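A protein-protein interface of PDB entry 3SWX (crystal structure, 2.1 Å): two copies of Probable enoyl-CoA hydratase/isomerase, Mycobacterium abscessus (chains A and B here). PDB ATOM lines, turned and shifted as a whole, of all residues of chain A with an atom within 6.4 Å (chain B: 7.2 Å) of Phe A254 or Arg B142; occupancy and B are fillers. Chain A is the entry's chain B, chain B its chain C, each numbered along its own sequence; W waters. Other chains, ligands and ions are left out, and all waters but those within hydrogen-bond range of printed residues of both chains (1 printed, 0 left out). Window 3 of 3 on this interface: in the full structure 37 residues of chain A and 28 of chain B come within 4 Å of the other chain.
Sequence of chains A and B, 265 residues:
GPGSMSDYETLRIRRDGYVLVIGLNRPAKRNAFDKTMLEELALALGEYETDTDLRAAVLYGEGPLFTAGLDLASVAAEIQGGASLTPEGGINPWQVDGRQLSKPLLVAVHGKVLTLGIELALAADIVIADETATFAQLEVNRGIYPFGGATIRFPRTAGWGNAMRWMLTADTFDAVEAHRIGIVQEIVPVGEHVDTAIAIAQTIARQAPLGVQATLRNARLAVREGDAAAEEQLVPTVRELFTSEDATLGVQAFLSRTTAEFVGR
ND2 of Asn B141 is in hydrogen-bond range of OE1 of Gln A207, 2.9 Å away.
The backbone carbonyl oxygen (O) of Val B140 is in hydrogen-bond range of the backbone NH (N) of Ala A208 (3.1 Å).
The backbone carbonyl oxygen (O) of Glu B139 sits at hydrogen-bond distance from the backbone NH (N) of Ile B144 (3.1 Å).
Gln A207 touches Ala B170.
CB of Ala A208 touches CA of Gly B143, at 3.6 Å.
CE1 of Phe A242 touches CG2 of Ile B144 (3.7 Å).
O of Asp A246 touches CA of Gly B143, at 3.7 Å.
O of Arg B142 touches O of Ala A247, at 3.8 Å.
Ala A247 touches Gly B143 (CA to O, 3.98 Å).
N of Val A251 touches O of Arg B142 (3.8 Å).
NH2 of Arg B142 touches CE1 of Phe A254 (3.3 Å).
Asn B141 touches Phe A262.
Phe A262 touches Gly B143.
Of chain B, only Arg B142 comes within 4 Å of Phe A254.
Of chain A, only Ala A247 (3.8 Å), Gly A250 (3.6 Å), Val A251 (3.8 Å) and Phe A254 (3.3 Å) come within 4 Å of Arg B142.
No residue of chain B comes within 4 Å of Ala A253.
Printed residues of chain A within 4 Å of Asn B141: Gln A207 (2.9 Å) and Phe A262 (3.3 Å).
Of the printed residues of chain B, Gly A250 touches Arg B142.
Glu B139 touches none of the printed residues of chain A.
Hydrophobic or aromatic side chains of chain B that line the printed part of chain A: Val B140, Ile B144 and Ala B170.
Printed residues of chain A that touch a printed residue of chain B: Gln A207, Ala A208, Phe A242, Asp A246, Ala A247, Gly A250, Val A251, Phe A254 and Phe A262.
Hydrophobic or aromatic side chains of chain A that line the printed part of chain B: Ala A208, Phe A242, Ala A247, Phe A254 and Phe A262.
Among the printed residues, 14 pairs touch across the chains.
Among the printed residues, no Asp or Glu carboxylate lies within 4 Å of a Lys or Arg side-chain nitrogen of the other chain.
No position is printed for both chains.
Of the 14 pairs that touch across the chains among the printed residues, none has its exchanged pair printed and touching as well.
Water W1 lies within hydrogen-bond range of the backbone carbonyl oxygen (O) of Asn B141 and the backbone carbonyl oxygen (O) of Gly A250.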
ATOM      1  N   GLN A 207     -14.365 -24.795  27.039  1.00  0.00           N
ATOM      2  CA  GLN A 207     -13.758 -23.883  26.072  1.00  0.00           C
ATOM      3  C   GLN A 207     -13.380 -22.561  26.744  1.00  0.00           C
ATOM      4  O   GLN A 207     -13.745 -22.301  27.898  1.00  0.00           O
ATOM      5  CB  GLN A 207     -14.705 -23.646  24.898  1.00  0.00           C
ATOM      6  CG  GLN A 207     -15.402 -24.930  24.428  1.00  0.00           C
ATOM      7  CD  GLN A 207     -14.428 -26.056  24.129  1.00  0.00           C
ATOM      8  OE1 GLN A 207     -13.406 -25.849  23.470  1.00  0.00           O
ATOM      9  NE2 GLN A 207     -14.748 -27.253  24.597  1.00  0.00           N
ATOM     10  N   ALA A 208     -12.635 -21.733  26.022  1.00  0.00           N
ATOM     11  CA  ALA A 208     -12.123 -20.488  26.597  1.00  0.00           C
ATOM     12  C   ALA A 208     -13.254 -19.483  26.741  1.00  0.00           C
ATOM     13  O   ALA A 208     -13.777 -19.043  25.723  1.00  0.00           O
ATOM     14  CB  ALA A 208     -11.028 -19.919  25.713  1.00  0.00           C
ATOM     15  N   PHE A 242      -5.661 -12.709  21.859  1.00  0.00           N
ATOM     16  CA  PHE A 242      -4.263 -13.200  21.784  1.00  0.00           C
ATOM     17  C   PHE A 242      -3.428 -12.709  22.960  1.00  0.00           C
ATOM     18  O   PHE A 242      -2.373 -13.251  23.267  1.00  0.00           O
ATOM     19  CB  PHE A 242      -3.577 -12.789  20.473  1.00  0.00           C
ATOM     20  CG  PHE A 242      -3.852 -13.725  19.336  1.00  0.00           C
ATOM     21  CD1 PHE A 242      -3.595 -15.085  19.462  1.00  0.00           C
ATOM     22  CD2 PHE A 242      -4.354 -13.251  18.135  1.00  0.00           C
ATOM     23  CE1 PHE A 242      -3.843 -15.956  18.417  1.00  0.00           C
ATOM     24  CE2 PHE A 242      -4.602 -14.121  17.087  1.00  0.00           C
ATOM     25  CZ  PHE A 242      -4.347 -15.473  17.228  1.00  0.00           C
ATOM     26  N   ASP A 246      -5.503 -17.284  28.427  1.00  0.00           N
ATOM     27  CA  ASP A 246      -6.133 -18.441  27.802  1.00  0.00           C
ATOM     28  C   ASP A 246      -5.662 -18.690  26.359  1.00  0.00           C
ATOM     29  O   ASP A 246      -5.583 -19.859  25.933  1.00  0.00           O
ATOM     30  CB  ASP A 246      -7.670 -18.326  27.888  1.00  0.00           C
ATOM     31  CG  ASP A 246      -8.204 -18.663  29.283  1.00  0.00           C
ATOM     32  OD1 ASP A 246      -7.436 -19.211  30.104  1.00  0.00           O
ATOM     33  OD2 ASP A 246      -9.388 -18.402  29.554  1.00  0.00           O
ATOM     34  N   ALA A 247      -5.346 -17.630  25.603  1.00  0.00           N
ATOM     35  CA  ALA A 247      -4.816 -17.833  24.236  1.00  0.00           C
ATOM     36  C   ALA A 247      -3.453 -18.561  24.256  1.00  0.00           C
ATOM     37  O   ALA A 247      -3.221 -19.496  23.484  1.00  0.00           O
ATOM     38  CB  ALA A 247      -4.729 -16.525  23.487  1.00  0.00           C
ATOM     39  N   THR A 248      -2.561 -18.157  25.154  1.00  0.00           N
ATOM     40  CA  THR A 248      -1.271 -18.853  25.285  1.00  0.00           C
ATOM     41  C   THR A 248      -1.495 -20.297  25.776  1.00  0.00           C
ATOM     42  O   THR A 248      -0.908 -21.247  25.234  1.00  0.00           O
ATOM     43  CB  THR A 248      -0.235 -18.066  26.165  1.00  0.00           C
ATOM     44  OG1 THR A 248      -0.701 -17.968  27.518  1.00  0.00           O
ATOM     45  CG2 THR A 248      -0.022 -16.675  25.626  1.00  0.00           C
ATOM     46  N   LEU A 249      -2.380 -20.479  26.751  1.00  0.00           N
ATOM     47  CA  LEU A 249      -2.742 -21.842  27.170  1.00  0.00           C
ATOM     48  C   LEU A 249      -3.300 -22.682  26.007  1.00  0.00           C
ATOM     49  O   LEU A 249      -2.890 -23.829  25.786  1.00  0.00           O
ATOM     50  CB  LEU A 249      -3.742 -21.810  28.335  1.00  0.00           C
ATOM     51  CG  LEU A 249      -3.191 -21.428  29.717  1.00  0.00           C
ATOM     52  CD1 LEU A 249      -4.324 -21.198  30.739  1.00  0.00           C
ATOM     53  CD2 LEU A 249      -2.199 -22.498  30.225  1.00  0.00           C
ATOM     54  N   GLY A 250      -4.234 -22.107  25.256  1.00  0.00           N
ATOM     55  CA  GLY A 250      -4.877 -22.830  24.157  1.00  0.00           C
ATOM     56  C   GLY A 250      -3.954 -23.153  22.990  1.00  0.00           C
ATOM     57  O   GLY A 250      -4.027 -24.227  22.410  1.00  0.00           O
ATOM     58  N   VAL A 251      -3.082 -22.221  22.635  1.00  0.00           N
ATOM     59  CA  VAL A 251      -2.154 -22.453  21.524  1.00  0.00           C
ATOM     60  C   VAL A 251      -1.068 -23.454  21.943  1.00  0.00           C
ATOM     61  O   VAL A 251      -0.732 -24.350  21.163  1.00  0.00           O
ATOM     62  CB  VAL A 251      -1.556 -21.124  20.968  1.00  0.00           C
ATOM     63  CG1 VAL A 251      -0.429 -21.401  19.955  1.00  0.00           C
ATOM     64  CG2 VAL A 251      -2.659 -20.271  20.338  1.00  0.00           C
ATOM     65  N   GLN A 252      -0.551 -23.343  23.173  1.00  0.00           N
ATOM     66  CA  GLN A 252       0.455 -24.313  23.662  1.00  0.00           C
ATOM     67  C   GLN A 252      -0.117 -25.730  23.729  1.00  0.00           C
ATOM     68  O   GLN A 252       0.572 -26.694  23.400  1.00  0.00           O
ATOM     69  CB  GLN A 252       1.033 -23.919  25.034  1.00  0.00           C
ATOM     70  N   ALA A 253      -1.376 -25.850  24.158  1.00  0.00           N
ATOM     71  CA  ALA A 253      -2.041 -27.149  24.252  1.00  0.00           C
ATOM     72  C   ALA A 253      -2.152 -27.800  22.874  1.00  0.00           C
ATOM     73  O   ALA A 253      -1.886 -28.992  22.698  1.00  0.00           O
ATOM     74  CB  ALA A 253      -3.434 -26.983  24.874  1.00  0.00           C
ATOM     75  N   PHE A 254      -2.554 -26.992  21.900  1.00  0.00           N
ATOM     76  CA  PHE A 254      -2.640 -27.427  20.517  1.00  0.00           C
ATOM     77  C   PHE A 254      -1.276 -27.920  20.016  1.00  0.00           C
ATOM     78  O   PHE A 254      -1.163 -29.052  19.541  1.00  0.00           O
ATOM     79  CB  PHE A 254      -3.165 -26.276  19.642  1.00  0.00           C
ATOM     80  CG  PHE A 254      -3.088 -26.545  18.171  1.00  0.00           C
ATOM     81  CD1 PHE A 254      -3.742 -27.641  17.614  1.00  0.00           C
ATOM     82  CD2 PHE A 254      -2.370 -25.697  17.332  1.00  0.00           C
ATOM     83  CE1 PHE A 254      -3.681 -27.887  16.242  1.00  0.00           C
ATOM     84  CE2 PHE A 254      -2.302 -25.945  15.968  1.00  0.00           C
ATOM     85  CZ  PHE A 254      -2.961 -27.043  15.420  1.00  0.00           C
ATOM     86  N   LEU A 255      -0.244 -27.083  20.139  1.00  0.00           N
ATOM     87  CA  LEU A 255       1.109 -27.431  19.647  1.00  0.00           C
ATOM     88  C   LEU A 255       1.667 -28.656  20.364  1.00  0.00           C
ATOM     89  O   LEU A 255       2.353 -29.472  19.753  1.00  0.00           O
ATOM     90  CB  LEU A 255       2.082 -26.252  19.816  1.00  0.00           C
ATOM     91  CG  LEU A 255       1.782 -25.027  18.951  1.00  0.00           C
ATOM     92  CD1 LEU A 255       2.647 -23.828  19.322  1.00  0.00           C
ATOM     93  CD2 LEU A 255       1.921 -25.381  17.470  1.00  0.00           C
ATOM     94  N   SER A 256       1.359 -28.770  21.657  1.00  0.00           N
ATOM     95  CA  SER A 256       1.798 -29.891  22.490  1.00  0.00           C
ATOM     96  C   SER A 256       0.880 -31.130  22.399  1.00  0.00           C
ATOM     97  O   SER A 256       1.155 -32.141  23.051  1.00  0.00           O
ATOM     98  CB  SER A 256       1.896 -29.436  23.964  1.00  0.00           C
ATOM     99  N   ARG A 257      -0.200 -31.055  21.613  1.00  0.00           N
ATOM    100  CA  ARG A 257      -1.202 -32.136  21.520  1.00  0.00           C
ATOM    101  C   ARG A 257      -1.661 -32.560  22.923  1.00  0.00           C
ATOM    102  O   ARG A 257      -1.696 -33.752  23.258  1.00  0.00           O
ATOM    103  CB  ARG A 257      -0.653 -33.335  20.723  1.00  0.00           C
ATOM    104  N   THR A 258      -1.978 -31.562  23.748  1.00  0.00           N
ATOM    105  CA  THR A 258      -2.450 -31.788  25.113  1.00  0.00           C
ATOM    106  C   THR A 258      -3.757 -31.024  25.296  1.00  0.00           C
ATOM    107  O   THR A 258      -4.206 -30.318  24.396  1.00  0.00           O
ATOM    108  CB  THR A 258      -1.404 -31.341  26.175  1.00  0.00           C
ATOM    109  OG1 THR A 258      -0.981 -29.997  25.911  1.00  0.00           O
ATOM    110  CG2 THR A 258      -0.192 -32.260  26.178  1.00  0.00           C
ATOM    111  N   ALA A 260      -6.232 -28.255  27.120  1.00  0.00           N
ATOM    112  CA  ALA A 260      -6.105 -26.971  27.814  1.00  0.00           C
ATOM    113  C   ALA A 260      -7.110 -26.839  28.969  1.00  0.00           C
ATOM    114  O   ALA A 260      -8.250 -27.255  28.845  1.00  0.00           O
ATOM    115  CB  ALA A 260      -6.266 -25.813  26.825  1.00  0.00           C
ATOM    116  N   PHE A 262      -8.671 -23.837  30.772  1.00  0.00           N
ATOM    117  CA  PHE A 262      -8.789 -22.371  30.670  1.00  0.00           C
ATOM    118  C   PHE A 262      -9.208 -21.732  31.982  1.00  0.00           C
ATOM    119  O   PHE A 262      -9.964 -22.327  32.740  1.00  0.00           O
ATOM    120  CB  PHE A 262      -9.787 -21.989  29.580  1.00  0.00           C
ATOM    121  CG  PHE A 262      -9.374 -22.437  28.204  1.00  0.00           C
ATOM    122  CD1 PHE A 262      -8.255 -21.882  27.586  1.00  0.00           C
ATOM    123  CD2 PHE A 262     -10.087 -23.410  27.540  1.00  0.00           C
ATOM    124  CE1 PHE A 262      -7.869 -22.295  26.331  1.00  0.00           C
ATOM    125  CE2 PHE A 262      -9.719 -23.821  26.259  1.00  0.00           C
ATOM    126  CZ  PHE A 262      -8.607 -23.272  25.660  1.00  0.00           C
ATOM    127  N   ALA B  68      -6.796 -27.658   7.530  1.00  0.00           N
ATOM    128  CA  ALA B  68      -6.700 -27.759   8.987  1.00  0.00           C
ATOM    129  C   ALA B  68      -6.847 -26.387   9.654  1.00  0.00           C
ATOM    130  O   ALA B  68      -6.692 -26.275  10.861  1.00  0.00           O
ATOM    131  CB  ALA B  68      -5.374 -28.406   9.387  1.00  0.00           C
ATOM    132  N   GLY B  69      -7.151 -25.343   8.885  1.00  0.00           N
ATOM    133  CA  GLY B  69      -7.428 -24.038   9.480  1.00  0.00           C
ATOM    134  C   GLY B  69      -6.244 -23.079   9.492  1.00  0.00           C
ATOM    135  O   GLY B  69      -5.467 -23.048   8.555  1.00  0.00           O
ATOM    136  N   LEU B  70      -6.123 -22.282  10.552  1.00  0.00           N
ATOM    137  CA  LEU B  70      -5.105 -21.241  10.621  1.00  0.00           C
ATOM    138  C   LEU B  70      -3.822 -21.849  11.154  1.00  0.00           C
ATOM    139  O   LEU B  70      -3.865 -22.589  12.121  1.00  0.00           O
ATOM    140  CB  LEU B  70      -5.563 -20.099  11.549  1.00  0.00           C
ATOM    141  CG  LEU B  70      -4.659 -18.849  11.604  1.00  0.00           C
ATOM    142  CD1 LEU B  70      -4.410 -18.226  10.210  1.00  0.00           C
ATOM    143  CD2 LEU B  70      -5.237 -17.802  12.546  1.00  0.00           C
ATOM    144  N   ASP B  71      -2.690 -21.549  10.530  1.00  0.00           N
ATOM    145  CA  ASP B  71      -1.405 -21.975  11.075  1.00  0.00           C
ATOM    146  C   ASP B  71      -1.094 -20.991  12.211  1.00  0.00           C
ATOM    147  O   ASP B  71      -0.455 -19.950  12.004  1.00  0.00           O
ATOM    148  CB  ASP B  71      -0.325 -21.994   9.991  1.00  0.00           C
ATOM    149  CG  ASP B  71       0.986 -22.622  10.464  1.00  0.00           C
ATOM    150  OD1 ASP B  71       1.252 -22.644  11.685  1.00  0.00           O
ATOM    151  OD2 ASP B  71       1.755 -23.086   9.591  1.00  0.00           O
ATOM    152  N   LEU B  72      -1.600 -21.338  13.400  1.00  0.00           N
ATOM    153  CA  LEU B  72      -1.605 -20.472  14.598  1.00  0.00           C
ATOM    154  C   LEU B  72      -0.617 -19.310  14.521  1.00  0.00           C
ATOM    155  O   LEU B  72      -1.032 -18.161  14.349  1.00  0.00           O
ATOM    156  CB  LEU B  72      -1.347 -21.315  15.843  1.00  0.00           C
ATOM    157  N   ALA B  73       0.672 -19.608  14.684  1.00  0.00           N
ATOM    158  CA  ALA B  73       1.769 -18.803  14.117  1.00  0.00           C
ATOM    159  C   ALA B  73       2.529 -19.814  13.283  1.00  0.00           C
ATOM    160  O   ALA B  73       2.420 -20.996  13.610  1.00  0.00           O
ATOM    161  CB  ALA B  73       2.673 -18.226  15.208  1.00  0.00           C
ATOM    162  N   LEU B 114     -11.664 -27.428   9.057  1.00  0.00           N
ATOM    163  CA  LEU B 114     -11.508 -26.808  10.368  1.00  0.00           C
ATOM    164  C   LEU B 114     -11.441 -25.288  10.308  1.00  0.00           C
ATOM    165  O   LEU B 114     -10.837 -24.718   9.389  1.00  0.00           O
ATOM    166  CB  LEU B 114     -10.242 -27.344  11.044  1.00  0.00           C
ATOM    167  CG  LEU B 114     -10.125 -28.869  11.124  1.00  0.00           C
ATOM    168  CD1 LEU B 114      -8.797 -29.233  11.748  1.00  0.00           C
ATOM    169  CD2 LEU B 114     -11.285 -29.512  11.929  1.00  0.00           C
ATOM    170  N   THR B 115     -12.045 -24.657  11.319  1.00  0.00           N
ATOM    171  CA  THR B 115     -11.963 -23.214  11.598  1.00  0.00           C
ATOM    172  C   THR B 115     -12.191 -22.352  10.345  1.00  0.00           C
ATOM    173  O   THR B 115     -13.312 -22.222   9.886  1.00  0.00           O
ATOM    174  CB  THR B 115     -10.617 -22.839  12.336  1.00  0.00           C
ATOM    175  OG1 THR B 115      -9.494 -23.154  11.508  1.00  0.00           O
ATOM    176  CG2 THR B 115     -10.476 -23.618  13.670  1.00  0.00           C
ATOM    177  N   LEU B 138     -13.140 -24.849  15.893  1.00  0.00           N
ATOM    178  CA  LEU B 138     -12.253 -25.128  17.010  1.00  0.00           C
ATOM    179  C   LEU B 138     -11.693 -23.905  17.728  1.00  0.00           C
ATOM    180  O   LEU B 138     -11.045 -24.068  18.754  1.00  0.00           O
ATOM    181  CB  LEU B 138     -11.074 -26.023  16.537  1.00  0.00           C
ATOM    182  CG  LEU B 138     -11.434 -27.448  16.076  1.00  0.00           C
ATOM    183  CD1 LEU B 138     -10.201 -28.120  15.509  1.00  0.00           C
ATOM    184  CD2 LEU B 138     -12.013 -28.305  17.218  1.00  0.00           C
ATOM    185  N   GLU B 139     -11.956 -22.699  17.211  1.00  0.00           N
ATOM    186  CA  GLU B 139     -11.299 -21.469  17.690  1.00  0.00           C
ATOM    187  C   GLU B 139     -11.452 -21.257  19.206  1.00  0.00           C
ATOM    188  O   GLU B 139     -10.469 -20.935  19.880  1.00  0.00           O
ATOM    189  CB  GLU B 139     -11.777 -20.233  16.928  1.00  0.00           C
ATOM    190  CG  GLU B 139     -11.400 -20.155  15.435  1.00  0.00           C
ATOM    191  CD  GLU B 139     -12.439 -20.753  14.508  1.00  0.00           C
ATOM    192  OE1 GLU B 139     -13.144 -21.716  14.889  1.00  0.00           O
ATOM    193  OE2 GLU B 139     -12.549 -20.265  13.375  1.00  0.00           O
ATOM    194  N   VAL B 140     -12.650 -21.474  19.760  1.00  0.00           N
ATOM    195  CA  VAL B 140     -12.797 -21.341  21.208  1.00  0.00           C
ATOM    196  C   VAL B 140     -12.033 -22.430  21.974  1.00  0.00           C
ATOM    197  O   VAL B 140     -11.720 -22.233  23.140  1.00  0.00           O
ATOM    198  CB  VAL B 140     -14.285 -21.274  21.690  1.00  0.00           C
ATOM    199  CG1 VAL B 140     -14.991 -20.021  21.105  1.00  0.00           C
ATOM    200  CG2 VAL B 140     -15.051 -22.585  21.394  1.00  0.00           C
ATOM    201  N   ASN B 141     -11.695 -23.552  21.326  1.00  0.00           N
ATOM    202  CA  ASN B 141     -10.903 -24.595  21.995  1.00  0.00           C
ATOM    203  C   ASN B 141      -9.426 -24.216  22.055  1.00  0.00           C
ATOM    204  O   ASN B 141      -8.668 -24.823  22.769  1.00  0.00           O
ATOM    205  CB  ASN B 141     -11.104 -25.948  21.305  1.00  0.00           C
ATOM    206  CG  ASN B 141     -10.461 -27.112  22.054  1.00  0.00           C
ATOM    207  OD1 ASN B 141      -9.442 -27.650  21.607  1.00  0.00           O
ATOM    208  ND2 ASN B 141     -11.047 -27.506  23.190  1.00  0.00           N
ATOM    209  N   ARG B 142      -9.032 -23.200  21.298  1.00  0.00           N
ATOM    210  CA  ARG B 142      -7.667 -22.734  21.253  1.00  0.00           C
ATOM    211  C   ARG B 142      -7.467 -21.357  21.888  1.00  0.00           C
ATOM    212  O   ARG B 142      -6.413 -20.729  21.734  1.00  0.00           O
ATOM    213  CB  ARG B 142      -7.208 -22.782  19.800  1.00  0.00           C
ATOM    214  CG  ARG B 142      -7.356 -24.212  19.268  1.00  0.00           C
ATOM    215  CD  ARG B 142      -7.066 -24.348  17.829  1.00  0.00           C
ATOM    216  NE  ARG B 142      -7.067 -25.741  17.412  1.00  0.00           N
ATOM    217  CZ  ARG B 142      -6.883 -26.128  16.150  1.00  0.00           C
ATOM    218  NH1 ARG B 142      -6.711 -25.213  15.186  1.00  0.00           N
ATOM    219  NH2 ARG B 142      -6.883 -27.420  15.837  1.00  0.00           N
ATOM    220  N   GLY B 143      -8.439 -20.911  22.671  1.00  0.00           N
ATOM    221  CA  GLY B 143      -8.308 -19.662  23.390  1.00  0.00           C
ATOM    222  C   GLY B 143      -8.708 -18.395  22.643  1.00  0.00           C
ATOM    223  O   GLY B 143      -8.621 -17.311  23.210  1.00  0.00           O
ATOM    224  N   ILE B 144      -9.143 -18.518  21.386  1.00  0.00           N
ATOM    225  CA  ILE B 144      -9.566 -17.362  20.590  1.00  0.00           C
ATOM    226  C   ILE B 144     -11.067 -17.507  20.241  1.00  0.00           C
ATOM    227  O   ILE B 144     -11.848 -17.984  21.064  1.00  0.00           O
ATOM    228  CB  ILE B 144      -8.628 -17.126  19.339  1.00  0.00           C
ATOM    229  CG1 ILE B 144      -8.508 -18.349  18.455  1.00  0.00           C
ATOM    230  CG2 ILE B 144      -7.237 -16.743  19.767  1.00  0.00           C
ATOM    231  CD1 ILE B 144      -8.073 -18.028  17.001  1.00  0.00           C
ATOM    232  N   TYR B 145     -11.484 -17.073  19.053  1.00  0.00           N
ATOM    233  CA  TYR B 145     -12.881 -17.217  18.616  1.00  0.00           C
ATOM    234  C   TYR B 145     -12.890 -17.138  17.093  1.00  0.00           C
ATOM    235  O   TYR B 145     -11.845 -16.844  16.510  1.00  0.00           O
ATOM    236  CB  TYR B 145     -13.764 -16.144  19.239  1.00  0.00           C
ATOM    237  CG  TYR B 145     -13.781 -14.844  18.454  1.00  0.00           C
ATOM    238  CD1 TYR B 145     -12.596 -14.175  18.170  1.00  0.00           C
ATOM    239  CD2 TYR B 145     -14.978 -14.281  18.011  1.00  0.00           C
ATOM    240  CE1 TYR B 145     -12.592 -12.974  17.469  1.00  0.00           C
ATOM    241  CE2 TYR B 145     -14.982 -13.086  17.303  1.00  0.00           C
ATOM    242  CZ  TYR B 145     -13.771 -12.449  17.030  1.00  0.00           C
ATOM    243  OH  TYR B 145     -13.727 -11.275  16.336  1.00  0.00           O
ATOM    244  N   ALA B 170     -17.118 -26.019  19.883  1.00  0.00           N
ATOM    245  CA  ALA B 170     -16.050 -26.585  19.061  1.00  0.00           C
ATOM    246  C   ALA B 170     -16.238 -28.076  18.709  1.00  0.00           C
ATOM    247  O   ALA B 170     -15.287 -28.738  18.285  1.00  0.00           O
ATOM    248  CB  ALA B 170     -14.676 -26.338  19.718  1.00  0.00           C
HETATM  249  O   HOH W   1      -6.143 -26.115  22.623  1.00  0.00           O
